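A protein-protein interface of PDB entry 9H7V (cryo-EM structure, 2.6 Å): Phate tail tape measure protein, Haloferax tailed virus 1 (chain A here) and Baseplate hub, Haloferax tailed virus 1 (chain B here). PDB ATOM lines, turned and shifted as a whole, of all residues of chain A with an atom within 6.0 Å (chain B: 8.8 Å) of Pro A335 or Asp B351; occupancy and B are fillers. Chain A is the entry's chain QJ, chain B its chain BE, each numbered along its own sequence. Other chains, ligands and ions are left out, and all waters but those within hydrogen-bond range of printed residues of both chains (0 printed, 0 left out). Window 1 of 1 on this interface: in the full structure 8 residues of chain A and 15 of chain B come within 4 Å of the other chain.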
ATOM      1  N   ARG A 330      -2.211 -18.282  30.618  1.00  0.00           N
ATOM      2  CA  ARG A 330      -1.301 -18.265  29.480  1.00  0.00           C
ATOM      3  C   ARG A 330      -2.072 -18.415  28.167  1.00  0.00           C
ATOM      4  O   ARG A 330      -1.679 -17.837  27.155  1.00  0.00           O
ATOM      5  CB  ARG A 330      -0.186 -19.308  29.650  1.00  0.00           C
ATOM      6  CG  ARG A 330      -0.659 -20.749  29.790  1.00  0.00           C
ATOM      7  CD  ARG A 330       0.419 -21.753  30.162  1.00  0.00           C
ATOM      8  NE  ARG A 330       0.896 -21.555  31.526  1.00  0.00           N
ATOM      9  CZ  ARG A 330       1.560 -22.445  32.260  1.00  0.00           C
ATOM     10  NH1 ARG A 330       1.936 -22.129  33.487  1.00  0.00           N
ATOM     11  NH2 ARG A 330       1.844 -23.645  31.780  1.00  0.00           N
ATOM     12  N   TYR A 331      -3.179 -19.169  28.210  1.00  0.00           N
ATOM     13  CA  TYR A 331      -3.951 -19.524  27.028  1.00  0.00           C
ATOM     14  C   TYR A 331      -5.059 -18.509  26.756  1.00  0.00           C
ATOM     15  O   TYR A 331      -5.482 -18.371  25.612  1.00  0.00           O
ATOM     16  CB  TYR A 331      -4.487 -20.953  27.141  1.00  0.00           C
ATOM     17  CG  TYR A 331      -3.438 -21.998  27.425  1.00  0.00           C
ATOM     18  CD1 TYR A 331      -2.399 -22.232  26.536  1.00  0.00           C
ATOM     19  CD2 TYR A 331      -3.472 -22.741  28.596  1.00  0.00           C
ATOM     20  CE1 TYR A 331      -1.428 -23.188  26.793  1.00  0.00           C
ATOM     21  CE2 TYR A 331      -2.511 -23.703  28.868  1.00  0.00           C
ATOM     22  CZ  TYR A 331      -1.485 -23.926  27.964  1.00  0.00           C
ATOM     23  OH  TYR A 331      -0.530 -24.866  28.220  1.00  0.00           O
ATOM     24  N   ARG A 332      -5.535 -17.823  27.806  1.00  0.00           N
ATOM     25  CA  ARG A 332      -6.566 -16.804  27.668  1.00  0.00           C
ATOM     26  C   ARG A 332      -5.983 -15.546  27.023  1.00  0.00           C
ATOM     27  O   ARG A 332      -6.683 -14.852  26.287  1.00  0.00           O
ATOM     28  CB  ARG A 332      -7.215 -16.474  29.016  1.00  0.00           C
ATOM     29  CG  ARG A 332      -8.043 -17.600  29.622  1.00  0.00           C
ATOM     30  CD  ARG A 332      -9.007 -17.146  30.706  1.00  0.00           C
ATOM     31  NE  ARG A 332      -8.449 -16.145  31.611  1.00  0.00           N
ATOM     32  CZ  ARG A 332      -7.799 -16.399  32.742  1.00  0.00           C
ATOM     33  NH1 ARG A 332      -7.337 -15.397  33.471  1.00  0.00           N
ATOM     34  NH2 ARG A 332      -7.613 -17.643  33.149  1.00  0.00           N
ATOM     35  N   SER A 333      -4.701 -15.273  27.298  1.00  0.00           N
ATOM     36  CA  SER A 333      -4.028 -14.059  26.859  1.00  0.00           C
ATOM     37  C   SER A 333      -3.439 -14.211  25.455  1.00  0.00           C
ATOM     38  O   SER A 333      -3.240 -13.210  24.770  1.00  0.00           O
ATOM     39  CB  SER A 333      -2.980 -13.626  27.855  1.00  0.00           C
ATOM     40  OG  SER A 333      -1.973 -14.617  27.997  1.00  0.00           O
ATOM     41  N   ASP A 334      -3.168 -15.460  25.044  1.00  0.00           N
ATOM     42  CA  ASP A 334      -2.479 -15.769  23.795  1.00  0.00           C
ATOM     43  C   ASP A 334      -3.235 -15.237  22.573  1.00  0.00           C
ATOM     44  O   ASP A 334      -2.598 -14.651  21.700  1.00  0.00           O
ATOM     45  CB  ASP A 334      -2.095 -17.250  23.687  1.00  0.00           C
ATOM     46  CG  ASP A 334      -1.557 -17.656  22.323  1.00  0.00           C
ATOM     47  OD1 ASP A 334      -0.504 -17.121  21.918  1.00  0.00           O
ATOM     48  OD2 ASP A 334      -2.201 -18.504  21.672  1.00  0.00           O
ATOM     49  N   PRO A 335      -4.575 -15.432  22.435  1.00  0.00           N
ATOM     50  CA  PRO A 335      -5.336 -14.839  21.330  1.00  0.00           C
ATOM     51  C   PRO A 335      -5.114 -13.347  21.080  1.00  0.00           C
ATOM     52  O   PRO A 335      -5.205 -12.900  19.938  1.00  0.00           O
ATOM     53  CB  PRO A 335      -6.797 -15.090  21.733  1.00  0.00           C
ATOM     54  CG  PRO A 335      -6.732 -16.385  22.502  1.00  0.00           C
ATOM     55  CD  PRO A 335      -5.432 -16.292  23.271  1.00  0.00           C
ATOM     56  N   SER A 336      -4.812 -12.595  22.148  1.00  0.00           N
ATOM     57  CA  SER A 336      -4.587 -11.160  22.059  1.00  0.00           C
ATOM     58  C   SER A 336      -3.129 -10.850  21.723  1.00  0.00           C
ATOM     59  O   SER A 336      -2.863  -9.891  21.000  1.00  0.00           O
ATOM     60  CB  SER A 336      -5.048 -10.450  23.303  1.00  0.00           C
ATOM     61  OG  SER A 336      -6.440 -10.645  23.509  1.00  0.00           O
ATOM     62  N   ARG A 337      -2.202 -11.664  22.245  1.00  0.00           N
ATOM     63  CA  ARG A 337      -0.782 -11.540  21.942  1.00  0.00           C
ATOM     64  C   ARG A 337      -0.530 -11.850  20.465  1.00  0.00           C
ATOM     65  O   ARG A 337       0.369 -11.270  19.860  1.00  0.00           O
ATOM     66  CB  ARG A 337       0.065 -12.392  22.898  1.00  0.00           C
ATOM     67  CG  ARG A 337       0.714 -11.610  24.034  1.00  0.00           C
ATOM     68  CD  ARG A 337      -0.266 -11.032  25.042  1.00  0.00           C
ATOM     69  NE  ARG A 337       0.325 -10.181  26.070  1.00  0.00           N
ATOM     70  CZ  ARG A 337       0.478  -8.860  25.992  1.00  0.00           C
ATOM     71  NH1 ARG A 337       1.016  -8.200  27.004  1.00  0.00           N
ATOM     72  NH2 ARG A 337       0.098  -8.198  24.913  1.00  0.00           N
ATOM     73  N   ARG A 338      -1.358 -12.741  19.901  1.00  0.00           N
ATOM     74  CA  ARG A 338      -1.351 -13.103  18.491  1.00  0.00           C
ATOM     75  C   ARG A 338      -1.748 -11.916  17.612  1.00  0.00           C
ATOM     76  O   ARG A 338      -1.433 -11.905  16.423  1.00  0.00           O
ATOM     77  CB  ARG A 338      -2.304 -14.280  18.249  1.00  0.00           C
ATOM     78  CG  ARG A 338      -1.623 -15.640  18.205  1.00  0.00           C
ATOM     79  CD  ARG A 338      -2.425 -16.745  18.866  1.00  0.00           C
ATOM     80  NE  ARG A 338      -3.776 -16.908  18.340  1.00  0.00           N
ATOM     81  CZ  ARG A 338      -4.727 -17.663  18.883  1.00  0.00           C
ATOM     82  NH1 ARG A 338      -5.916 -17.730  18.311  1.00  0.00           N
ATOM     83  NH2 ARG A 338      -4.492 -18.353  19.986  1.00  0.00           N
ATOM     84  N   ARG A 339      -2.430 -10.924  18.203  1.00  0.00           N
ATOM     85  CA  ARG A 339      -2.977  -9.792  17.468  1.00  0.00           C
ATOM     86  C   ARG A 339      -2.288  -8.489  17.874  1.00  0.00           C
ATOM     87  O   ARG A 339      -2.792  -7.403  17.585  1.00  0.00           O
ATOM     88  CB  ARG A 339      -4.493  -9.715  17.672  1.00  0.00           C
ATOM     89  CG  ARG A 339      -5.255 -10.888  17.074  1.00  0.00           C
ATOM     90  CD  ARG A 339      -6.734 -10.829  17.386  1.00  0.00           C
ATOM     91  NE  ARG A 339      -7.453  -9.800  16.649  1.00  0.00           N
ATOM     92  CZ  ARG A 339      -8.748  -9.534  16.777  1.00  0.00           C
ATOM     93  NH1 ARG A 339      -9.298  -8.575  16.052  1.00  0.00           N
ATOM     94  NH2 ARG A 339      -9.495 -10.220  17.627  1.00  0.00           N
ATOM     95  N   ILE A 341      -1.720  -6.322  20.745  1.00  0.00           N
ATOM     96  CA  ILE A 341      -2.175  -5.955  22.079  1.00  0.00           C
ATOM     97  C   ILE A 341      -3.710  -5.981  22.084  1.00  0.00           C
ATOM     98  O   ILE A 341      -4.360  -5.407  21.211  1.00  0.00           O
ATOM     99  CB  ILE A 341      -1.596  -4.586  22.512  1.00  0.00           C
ATOM    100  CG1 ILE A 341      -0.063  -4.576  22.507  1.00  0.00           C
ATOM    101  CG2 ILE A 341      -2.146  -4.160  23.869  1.00  0.00           C
ATOM    102  CD1 ILE A 341       0.555  -3.241  22.146  1.00  0.00           C
ATOM    103  OXT ILE A 341      -4.333  -6.585  22.957  1.00  0.00           O
ATOM    104  N   PRO B  49      -7.412 -10.345  10.457  1.00  0.00           N
ATOM    105  CA  PRO B  49      -7.500  -9.883  11.844  1.00  0.00           C
ATOM    106  C   PRO B  49      -6.723 -10.766  12.823  1.00  0.00           C
ATOM    107  O   PRO B  49      -6.358 -10.308  13.903  1.00  0.00           O
ATOM    108  CB  PRO B  49      -9.002  -9.909  12.166  1.00  0.00           C
ATOM    109  CG  PRO B  49      -9.681  -9.867  10.814  1.00  0.00           C
ATOM    110  CD  PRO B  49      -8.740 -10.583   9.866  1.00  0.00           C
ATOM    111  N   PHE B  50      -6.438 -12.010  12.409  1.00  0.00           N
ATOM    112  CA  PHE B  50      -6.012 -13.072  13.310  1.00  0.00           C
ATOM    113  C   PHE B  50      -4.628 -13.600  12.935  1.00  0.00           C
ATOM    114  O   PHE B  50      -4.308 -13.767  11.755  1.00  0.00           O
ATOM    115  CB  PHE B  50      -7.055 -14.192  13.328  1.00  0.00           C
ATOM    116  CG  PHE B  50      -8.454 -13.749  13.674  1.00  0.00           C
ATOM    117  CD1 PHE B  50      -8.845 -13.612  14.998  1.00  0.00           C
ATOM    118  CD2 PHE B  50      -9.379 -13.466  12.678  1.00  0.00           C
ATOM    119  CE1 PHE B  50     -10.130 -13.198  15.321  1.00  0.00           C
ATOM    120  CE2 PHE B  50     -10.664 -13.051  13.002  1.00  0.00           C
ATOM    121  CZ  PHE B  50     -11.037 -12.918  14.322  1.00  0.00           C
ATOM    122  N   GLY B  51      -3.833 -13.893  13.972  1.00  0.00           N
ATOM    123  CA  GLY B  51      -2.466 -14.363  13.817  1.00  0.00           C
ATOM    124  C   GLY B  51      -2.397 -15.855  13.504  1.00  0.00           C
ATOM    125  O   GLY B  51      -3.063 -16.660  14.152  1.00  0.00           O
ATOM    126  N   TYR B  53      -0.396 -19.276  13.711  1.00  0.00           N
ATOM    127  CA  TYR B  53       0.489 -19.803  14.737  1.00  0.00           C
ATOM    128  C   TYR B  53       0.603 -21.323  14.653  1.00  0.00           C
ATOM    129  O   TYR B  53      -0.262 -21.992  14.089  1.00  0.00           O
ATOM    130  CB  TYR B  53       0.069 -19.312  16.128  1.00  0.00           C
ATOM    131  CG  TYR B  53      -1.165 -19.953  16.712  1.00  0.00           C
ATOM    132  CD1 TYR B  53      -2.435 -19.533  16.342  1.00  0.00           C
ATOM    133  CD2 TYR B  53      -1.064 -20.965  17.657  1.00  0.00           C
ATOM    134  CE1 TYR B  53      -3.571 -20.114  16.883  1.00  0.00           C
ATOM    135  CE2 TYR B  53      -2.191 -21.557  18.205  1.00  0.00           C
ATOM    136  CZ  TYR B  53      -3.449 -21.128  17.817  1.00  0.00           C
ATOM    137  OH  TYR B  53      -4.565 -21.703  18.353  1.00  0.00           O
ATOM    138  N   GLU B 111       5.881 -22.490  20.736  1.00  0.00           N
ATOM    139  CA  GLU B 111       4.870 -21.699  20.056  1.00  0.00           C
ATOM    140  C   GLU B 111       5.554 -20.727  19.099  1.00  0.00           C
ATOM    141  O   GLU B 111       6.519 -20.060  19.468  1.00  0.00           O
ATOM    142  CB  GLU B 111       3.977 -20.991  21.075  1.00  0.00           C
ATOM    143  CG  GLU B 111       2.828 -20.225  20.445  1.00  0.00           C
ATOM    144  CD  GLU B 111       1.571 -20.082  21.286  1.00  0.00           C
ATOM    145  OE1 GLU B 111       1.679 -20.046  22.530  1.00  0.00           O
ATOM    146  OE2 GLU B 111       0.479 -20.002  20.690  1.00  0.00           O
ATOM    147  N   TYR B 113       4.866 -17.784  15.766  1.00  0.00           N
ATOM    148  CA  TYR B 113       4.030 -16.886  14.980  1.00  0.00           C
ATOM    149  C   TYR B 113       4.618 -16.790  13.567  1.00  0.00           C
ATOM    150  O   TYR B 113       5.743 -17.236  13.351  1.00  0.00           O
ATOM    151  CB  TYR B 113       3.908 -15.524  15.677  1.00  0.00           C
ATOM    152  CG  TYR B 113       3.212 -15.446  17.021  1.00  0.00           C
ATOM    153  CD1 TYR B 113       2.461 -16.493  17.542  1.00  0.00           C
ATOM    154  CD2 TYR B 113       3.264 -14.271  17.762  1.00  0.00           C
ATOM    155  CE1 TYR B 113       1.824 -16.391  18.772  1.00  0.00           C
ATOM    156  CE2 TYR B 113       2.626 -14.147  18.988  1.00  0.00           C
ATOM    157  CZ  TYR B 113       1.901 -15.211  19.495  1.00  0.00           C
ATOM    158  OH  TYR B 113       1.269 -15.103  20.699  1.00  0.00           O
ATOM    159  N   GLN B 117       2.498 -11.088  11.349  1.00  0.00           N
ATOM    160  CA  GLN B 117       2.932 -10.268  12.472  1.00  0.00           C
ATOM    161  C   GLN B 117       3.601  -8.983  11.987  1.00  0.00           C
ATOM    162  O   GLN B 117       3.578  -7.979  12.696  1.00  0.00           O
ATOM    163  CB  GLN B 117       3.870 -11.056  13.391  1.00  0.00           C
ATOM    164  CG  GLN B 117       3.197 -12.199  14.142  1.00  0.00           C
ATOM    165  CD  GLN B 117       2.030 -11.779  15.004  1.00  0.00           C
ATOM    166  OE1 GLN B 117       2.060 -10.752  15.678  1.00  0.00           O
ATOM    167  NE2 GLN B 117       0.983 -12.588  14.997  1.00  0.00           N
ATOM    168  N   ARG B 120       1.005  -6.511  11.163  1.00  0.00           N
ATOM    169  CA  ARG B 120       0.279  -6.224  12.392  1.00  0.00           C
ATOM    170  C   ARG B 120       1.010  -5.161  13.212  1.00  0.00           C
ATOM    171  O   ARG B 120       0.370  -4.311  13.832  1.00  0.00           O
ATOM    172  CB  ARG B 120       0.147  -7.528  13.186  1.00  0.00           C
ATOM    173  CG  ARG B 120      -0.767  -7.471  14.403  1.00  0.00           C
ATOM    174  CD  ARG B 120      -2.252  -7.717  14.183  1.00  0.00           C
ATOM    175  NE  ARG B 120      -2.692  -8.596  13.098  1.00  0.00           N
ATOM    176  CZ  ARG B 120      -2.387  -9.886  12.942  1.00  0.00           C
ATOM    177  NH1 ARG B 120      -2.877 -10.551  11.910  1.00  0.00           N
ATOM    178  NH2 ARG B 120      -1.580 -10.506  13.785  1.00  0.00           N
ATOM    179  N   GLU B 225     -23.090  -8.416  18.846  1.00  0.00           N
ATOM    180  CA  GLU B 225     -22.343  -7.171  18.737  1.00  0.00           C
ATOM    181  C   GLU B 225     -23.058  -6.168  17.825  1.00  0.00           C
ATOM    182  O   GLU B 225     -22.715  -4.987  17.830  1.00  0.00           O
ATOM    183  CB  GLU B 225     -20.909  -7.459  18.277  1.00  0.00           C
ATOM    184  CG  GLU B 225     -19.937  -6.322  18.547  1.00  0.00           C
ATOM    185  CD  GLU B 225     -18.474  -6.590  18.228  1.00  0.00           C
ATOM    186  OE1 GLU B 225     -18.124  -7.756  17.944  1.00  0.00           O
ATOM    187  OE2 GLU B 225     -17.679  -5.627  18.270  1.00  0.00           O
ATOM    188  N   LYS B 346     -14.635 -15.342  10.653  1.00  0.00           N
ATOM    189  CA  LYS B 346     -14.095 -15.636  11.972  1.00  0.00           C
ATOM    190  C   LYS B 346     -14.205 -14.397  12.854  1.00  0.00           C
ATOM    191  O   LYS B 346     -13.868 -13.293  12.428  1.00  0.00           O
ATOM    192  CB  LYS B 346     -12.652 -16.147  11.909  1.00  0.00           C
ATOM    193  CG  LYS B 346     -12.159 -16.791  13.200  1.00  0.00           C
ATOM    194  CD  LYS B 346     -10.727 -17.278  13.155  1.00  0.00           C
ATOM    195  CE  LYS B 346     -10.370 -18.170  14.327  1.00  0.00           C
ATOM    196  NZ  LYS B 346     -10.364 -17.434  15.614  1.00  0.00           N
ATOM    197  N   ARG B 347     -14.693 -14.609  14.081  1.00  0.00           N
ATOM    198  CA  ARG B 347     -14.755 -13.576  15.101  1.00  0.00           C
ATOM    199  C   ARG B 347     -14.203 -14.134  16.408  1.00  0.00           C
ATOM    200  O   ARG B 347     -14.409 -15.305  16.724  1.00  0.00           O
ATOM    201  CB  ARG B 347     -16.179 -13.025  15.241  1.00  0.00           C
ATOM    202  CG  ARG B 347     -16.629 -12.231  14.025  1.00  0.00           C
ATOM    203  CD  ARG B 347     -17.891 -11.411  14.157  1.00  0.00           C
ATOM    204  NE  ARG B 347     -18.207 -10.910  12.826  1.00  0.00           N
ATOM    205  CZ  ARG B 347     -19.367 -10.384  12.453  1.00  0.00           C
ATOM    206  NH1 ARG B 347     -19.530  -9.974  11.207  1.00  0.00           N
ATOM    207  NH2 ARG B 347     -20.363 -10.276  13.315  1.00  0.00           N
ATOM    208  N   GLY B 348     -13.497 -13.274  17.151  1.00  0.00           N
ATOM    209  CA  GLY B 348     -12.939 -13.632  18.444  1.00  0.00           C
ATOM    210  C   GLY B 348     -13.999 -13.601  19.542  1.00  0.00           C
ATOM    211  O   GLY B 348     -15.192 -13.718  19.267  1.00  0.00           O
ATOM    212  N   ASP B 349     -13.537 -13.448  20.787  1.00  0.00           N
ATOM    213  CA  ASP B 349     -14.417 -13.321  21.939  1.00  0.00           C
ATOM    214  C   ASP B 349     -13.947 -12.160  22.818  1.00  0.00           C
ATOM    215  O   ASP B 349     -14.207 -11.008  22.476  1.00  0.00           O
ATOM    216  CB  ASP B 349     -14.674 -14.668  22.625  1.00  0.00           C
ATOM    217  CG  ASP B 349     -13.457 -15.573  22.706  1.00  0.00           C
ATOM    218  OD1 ASP B 349     -12.418 -15.118  23.230  1.00  0.00           O
ATOM    219  OD2 ASP B 349     -13.556 -16.726  22.239  1.00  0.00           O
ATOM    220  N   VAL B 350     -13.263 -12.462  23.934  1.00  0.00           N
ATOM    221  CA  VAL B 350     -12.719 -11.448  24.833  1.00  0.00           C
ATOM    222  C   VAL B 350     -11.628 -10.683  24.084  1.00  0.00           C
ATOM    223  O   VAL B 350     -11.426  -9.488  24.295  1.00  0.00           O
ATOM    224  CB  VAL B 350     -12.192 -12.060  26.149  1.00  0.00           C
ATOM    225  CG1 VAL B 350     -11.546 -11.027  27.063  1.00  0.00           C
ATOM    226  CG2 VAL B 350     -13.281 -12.807  26.902  1.00  0.00           C
ATOM    227  N   ASP B 351     -10.961 -11.420  23.193  1.00  0.00           N
ATOM    228  CA  ASP B 351      -9.916 -10.972  22.291  1.00  0.00           C
ATOM    229  C   ASP B 351     -10.400  -9.817  21.412  1.00  0.00           C
ATOM    230  O   ASP B 351      -9.654  -8.862  21.201  1.00  0.00           O
ATOM    231  CB  ASP B 351      -9.427 -12.179  21.487  1.00  0.00           C
ATOM    232  CG  ASP B 351      -8.407 -11.854  20.417  1.00  0.00           C
ATOM    233  OD1 ASP B 351      -7.475 -11.076  20.703  1.00  0.00           O
ATOM    234  OD2 ASP B 351      -8.560 -12.386  19.302  1.00  0.00           O
ATOM    235  N   ASP B 352     -11.635  -9.920  20.900  1.00  0.00           N
ATOM    236  CA  ASP B 352     -12.236  -8.900  20.052  1.00  0.00           C
ATOM    237  C   ASP B 352     -12.506  -7.627  20.852  1.00  0.00           C
ATOM    238  O   ASP B 352     -12.332  -6.529  20.326  1.00  0.00           O
ATOM    239  CB  ASP B 352     -13.494  -9.412  19.339  1.00  0.00           C
ATOM    240  CG  ASP B 352     -13.265  -9.945  17.931  1.00  0.00           C
ATOM    241  OD1 ASP B 352     -12.165  -9.728  17.379  1.00  0.00           O
ATOM    242  OD2 ASP B 352     -14.201 -10.567  17.388  1.00  0.00           O
ATOM    243  N   ILE B 353     -12.930  -7.789  22.115  1.00  0.00           N
ATOM    244  CA  ILE B 353     -13.207  -6.673  23.011  1.00  0.00           C
ATOM    245  C   ILE B 353     -11.908  -5.918  23.284  1.00  0.00           C
ATOM    246  O   ILE B 353     -11.864  -4.696  23.147  1.00  0.00           O
ATOM    247  CB  ILE B 353     -13.892  -7.142  24.315  1.00  0.00           C
ATOM    248  CG1 ILE B 353     -15.210  -7.871  24.037  1.00  0.00           C
ATOM    249  CG2 ILE B 353     -14.086  -5.977  25.280  1.00  0.00           C
ATOM    250  CD1 ILE B 353     -15.731  -8.690  25.195  1.00  0.00           C
ATOM    251  N   LEU B 354     -10.864  -6.670  23.656  1.00  0.00           N
ATOM    252  CA  LEU B 354      -9.586  -6.112  24.071  1.00  0.00           C
ATOM    253  C   LEU B 354      -8.895  -5.413  22.902  1.00  0.00           C
ATOM    254  O   LEU B 354      -8.262  -4.381  23.105  1.00  0.00           O
ATOM    255  CB  LEU B 354      -8.702  -7.218  24.660  1.00  0.00           C
ATOM    256  CG  LEU B 354      -9.034  -7.663  26.084  1.00  0.00           C
ATOM    257  CD1 LEU B 354      -8.310  -8.957  26.422  1.00  0.00           C
ATOM    258  CD2 LEU B 354      -8.688  -6.584  27.102  1.00  0.00           C
ATOM    259  N   SER B 355      -9.034  -5.972  21.692  1.00  0.00           N
ATOM    260  CA  SER B 355      -8.389  -5.414  20.513  1.00  0.00           C
ATOM    261  C   SER B 355      -9.082  -4.135  20.041  1.00  0.00           C
ATOM    262  O   SER B 355      -8.432  -3.285  19.435  1.00  0.00           O
ATOM    263  CB  SER B 355      -8.238  -6.427  19.405  1.00  0.00           C
ATOM    264  OG  SER B 355      -9.491  -6.989  19.050  1.00  0.00           O
ATOM    265  N   GLU B 356     -10.386  -4.000  20.326  1.00  0.00           N
ATOM    266  CA  GLU B 356     -11.132  -2.795  19.988  1.00  0.00           C
ATOM    267  C   GLU B 356     -10.762  -1.660  20.941  1.00  0.00           C
ATOM    268  O   GLU B 356     -10.642  -0.515  20.508  1.00  0.00           O
ATOM    269  CB  GLU B 356     -12.644  -3.041  19.981  1.00  0.00           C
ATOM    270  CG  GLU B 356     -13.157  -3.758  18.741  1.00  0.00           C
ATOM    271  CD  GLU B 356     -13.004  -3.033  17.413  1.00  0.00           C
ATOM    272  OE1 GLU B 356     -11.934  -3.172  16.782  1.00  0.00           O
ATOM    273  OE2 GLU B 356     -13.952  -2.329  17.011  1.00  0.00           O
ATOM    274  N   LEU B 357     -10.594  -1.994  22.229  1.00  0.00           N
ATOM    275  CA  LEU B 357     -10.186  -1.034  23.244  1.00  0.00           C
ATOM    276  C   LEU B 357      -8.754  -0.581  22.973  1.00  0.00           C
ATOM    277  O   LEU B 357      -8.463   0.611  23.045  1.00  0.00           O
ATOM    278  CB  LEU B 357     -10.317  -1.658  24.639  1.00  0.00           C
ATOM    279  CG  LEU B 357     -11.739  -1.856  25.168  1.00  0.00           C
ATOM    280  CD1 LEU B 357     -11.718  -2.609  26.489  1.00  0.00           C
ATOM    281  CD2 LEU B 357     -12.463  -0.527  25.332  1.00  0.00           C
ATOM    282  N   SER B 358      -7.890  -1.549  22.638  1.00  0.00           N
ATOM    283  CA  SER B 358      -6.479  -1.333  22.354  1.00  0.00           C
ATOM    284  C   SER B 358      -6.298  -0.372  21.181  1.00  0.00           C
ATOM    285  O   SER B 358      -5.490   0.552  21.263  1.00  0.00           O
ATOM    286  CB  SER B 358      -5.787  -2.646  22.107  1.00  0.00           C
ATOM    287  OG  SER B 358      -4.410  -2.453  21.827  1.00  0.00           O
ATOM    288  N   GLU B 359      -7.065  -0.604  20.106  1.00  0.00           N
ATOM    289  CA  GLU B 359      -7.018   0.193  18.890  1.00  0.00           C
ATOM    290  C   GLU B 359      -7.523   1.609  19.168  1.00  0.00           C
ATOM    291  O   GLU B 359      -6.963   2.572  18.645  1.00  0.00           O
ATOM    292  CB  GLU B 359      -7.834  -0.488  17.790  1.00  0.00           C
ATOM    293  CG  GLU B 359      -7.625   0.101  16.407  1.00  0.00           C
ATOM    294  CD  GLU B 359      -8.836  -0.045  15.502  1.00  0.00           C
ATOM    295  OE1 GLU B 359      -9.743   0.808  15.587  1.00  0.00           O
ATOM    296  OE2 GLU B 359      -8.880  -1.023  14.730  1.00  0.00           O
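The backbone carbonyl oxygen of Pro A335 lies close to the side-chain carboxylate of Asp B351, at 3.0 Å.
The side-chain carboxylate (OD1) of Asp B351 lies within hydrogen-bond range of the side-chain hydroxyl (OG) of Ser A336, at 3.0 Å.
The side-chain carboxylate of Asp A334 lies close to the side-chain carboxylate of Glu B111 (3.2 Å).
NE of Arg A339 lies within hydrogen-bond range of O of Pro B49 (3.0 Å).
The side-chain hydroxyl (OH) of Tyr B113 sits at hydrogen-bond distance from the side-chain carboxylate (OD1) of Asp A334 (2.9 Å).
OD1 of Asp B352 lies within salt-bridge range of NH2 of Arg A339, 2.7 Å away.
O of Arg A338 is in hydrogen-bond range of NH2 of Arg B120, at 3.0 Å.
NH2 of Arg A339 is in salt-bridge range of OD2 of Asp B351.
The side-chain hydroxyl of Ser B355 sits at hydrogen-bond distance from the guanidinium group of Arg A339, at 3.4 Å.
The side-chain amide nitrogen (NE2) of Gln B117 lies within hydrogen-bond range of the backbone carbonyl oxygen (O) of Arg A338 (2.9 Å).
The chain-end carboxylate of Ile A341 is in hydrogen-bond range of the side-chain hydroxyl of Ser B358 (3.0 Å).
NH2 of Arg A338 lies within salt-bridge range of OD2 of Asp A334, 2.8 Å away.
O of Asp B351 lies within hydrogen-bond range of OG of Ser B355 (2.9 Å).
The backbone carbonyl oxygen (O) of Asp B352 is in hydrogen-bond range of the side-chain hydroxyl (OG) of Ser B355 (3.1 Å).
N of Gly B348 sits at hydrogen-bond distance from OD2 of Asp B352.
Ser A336 touches Leu B354.
CB of Arg A337 touches OH of Tyr B113 (3.7 Å).
Arg A338 touches Gly B51 (O to CA, 3.7 Å).
CZ of Arg A338 touches CE1 of Tyr B53 (3.4 Å).
CE1 of Tyr B113 touches CG of Arg A338, at 3.6 Å.
Arg A339 touches Phe B50.
Arg A339 touches Arg B120.
Asp A334 touches two residues of chain B.
Of chain B, only Asp B351 comes within 4 Å of Pro A335.
Of chain B, only Asp B351 (3.0 Å) and Leu B354 (3.9 Å) come within 4 Å of Ser A336.
Printed residues of chain B within 4 Å of Arg A339: Pro B49, Phe B50, Arg B120, Asp B351, Asp B352 and Ser B355.
Of the printed residues of chain A, Arg B120 touches Arg A338 and Arg A339.
Lys B346 touches none of the printed residues of chain A.
Printed residues of chain A within 4 Å of Asp B351: Pro A335 (3.0 Å), Ser A336 (3.0 Å) and Arg A339 (2.9 Å).
Of the printed residues of chain A, Ser B358 touches Ile A341.
The nearest residue of chain B that does not touch Pro A335 is Asp B349 (5.8 Å).
The nearest residue of chain A that does not touch Asp B351 is Arg A337 (5.5 Å).
The nearest printed residue of chain A that does not touch Tyr B53 is Asp A334 (4.6 Å).
Of the 11 printed residues of chain A, 7 touch a printed residue of chain B.
Of the 23 printed residues of chain B, 13 touch a printed residue of chain A.
Hydrophobic or aromatic side chains of chain B that line the printed part of chain A: Phe B50, Tyr B53, Tyr B113 and Leu B354.
Among the printed residues, 18 pairs touch across the chains.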
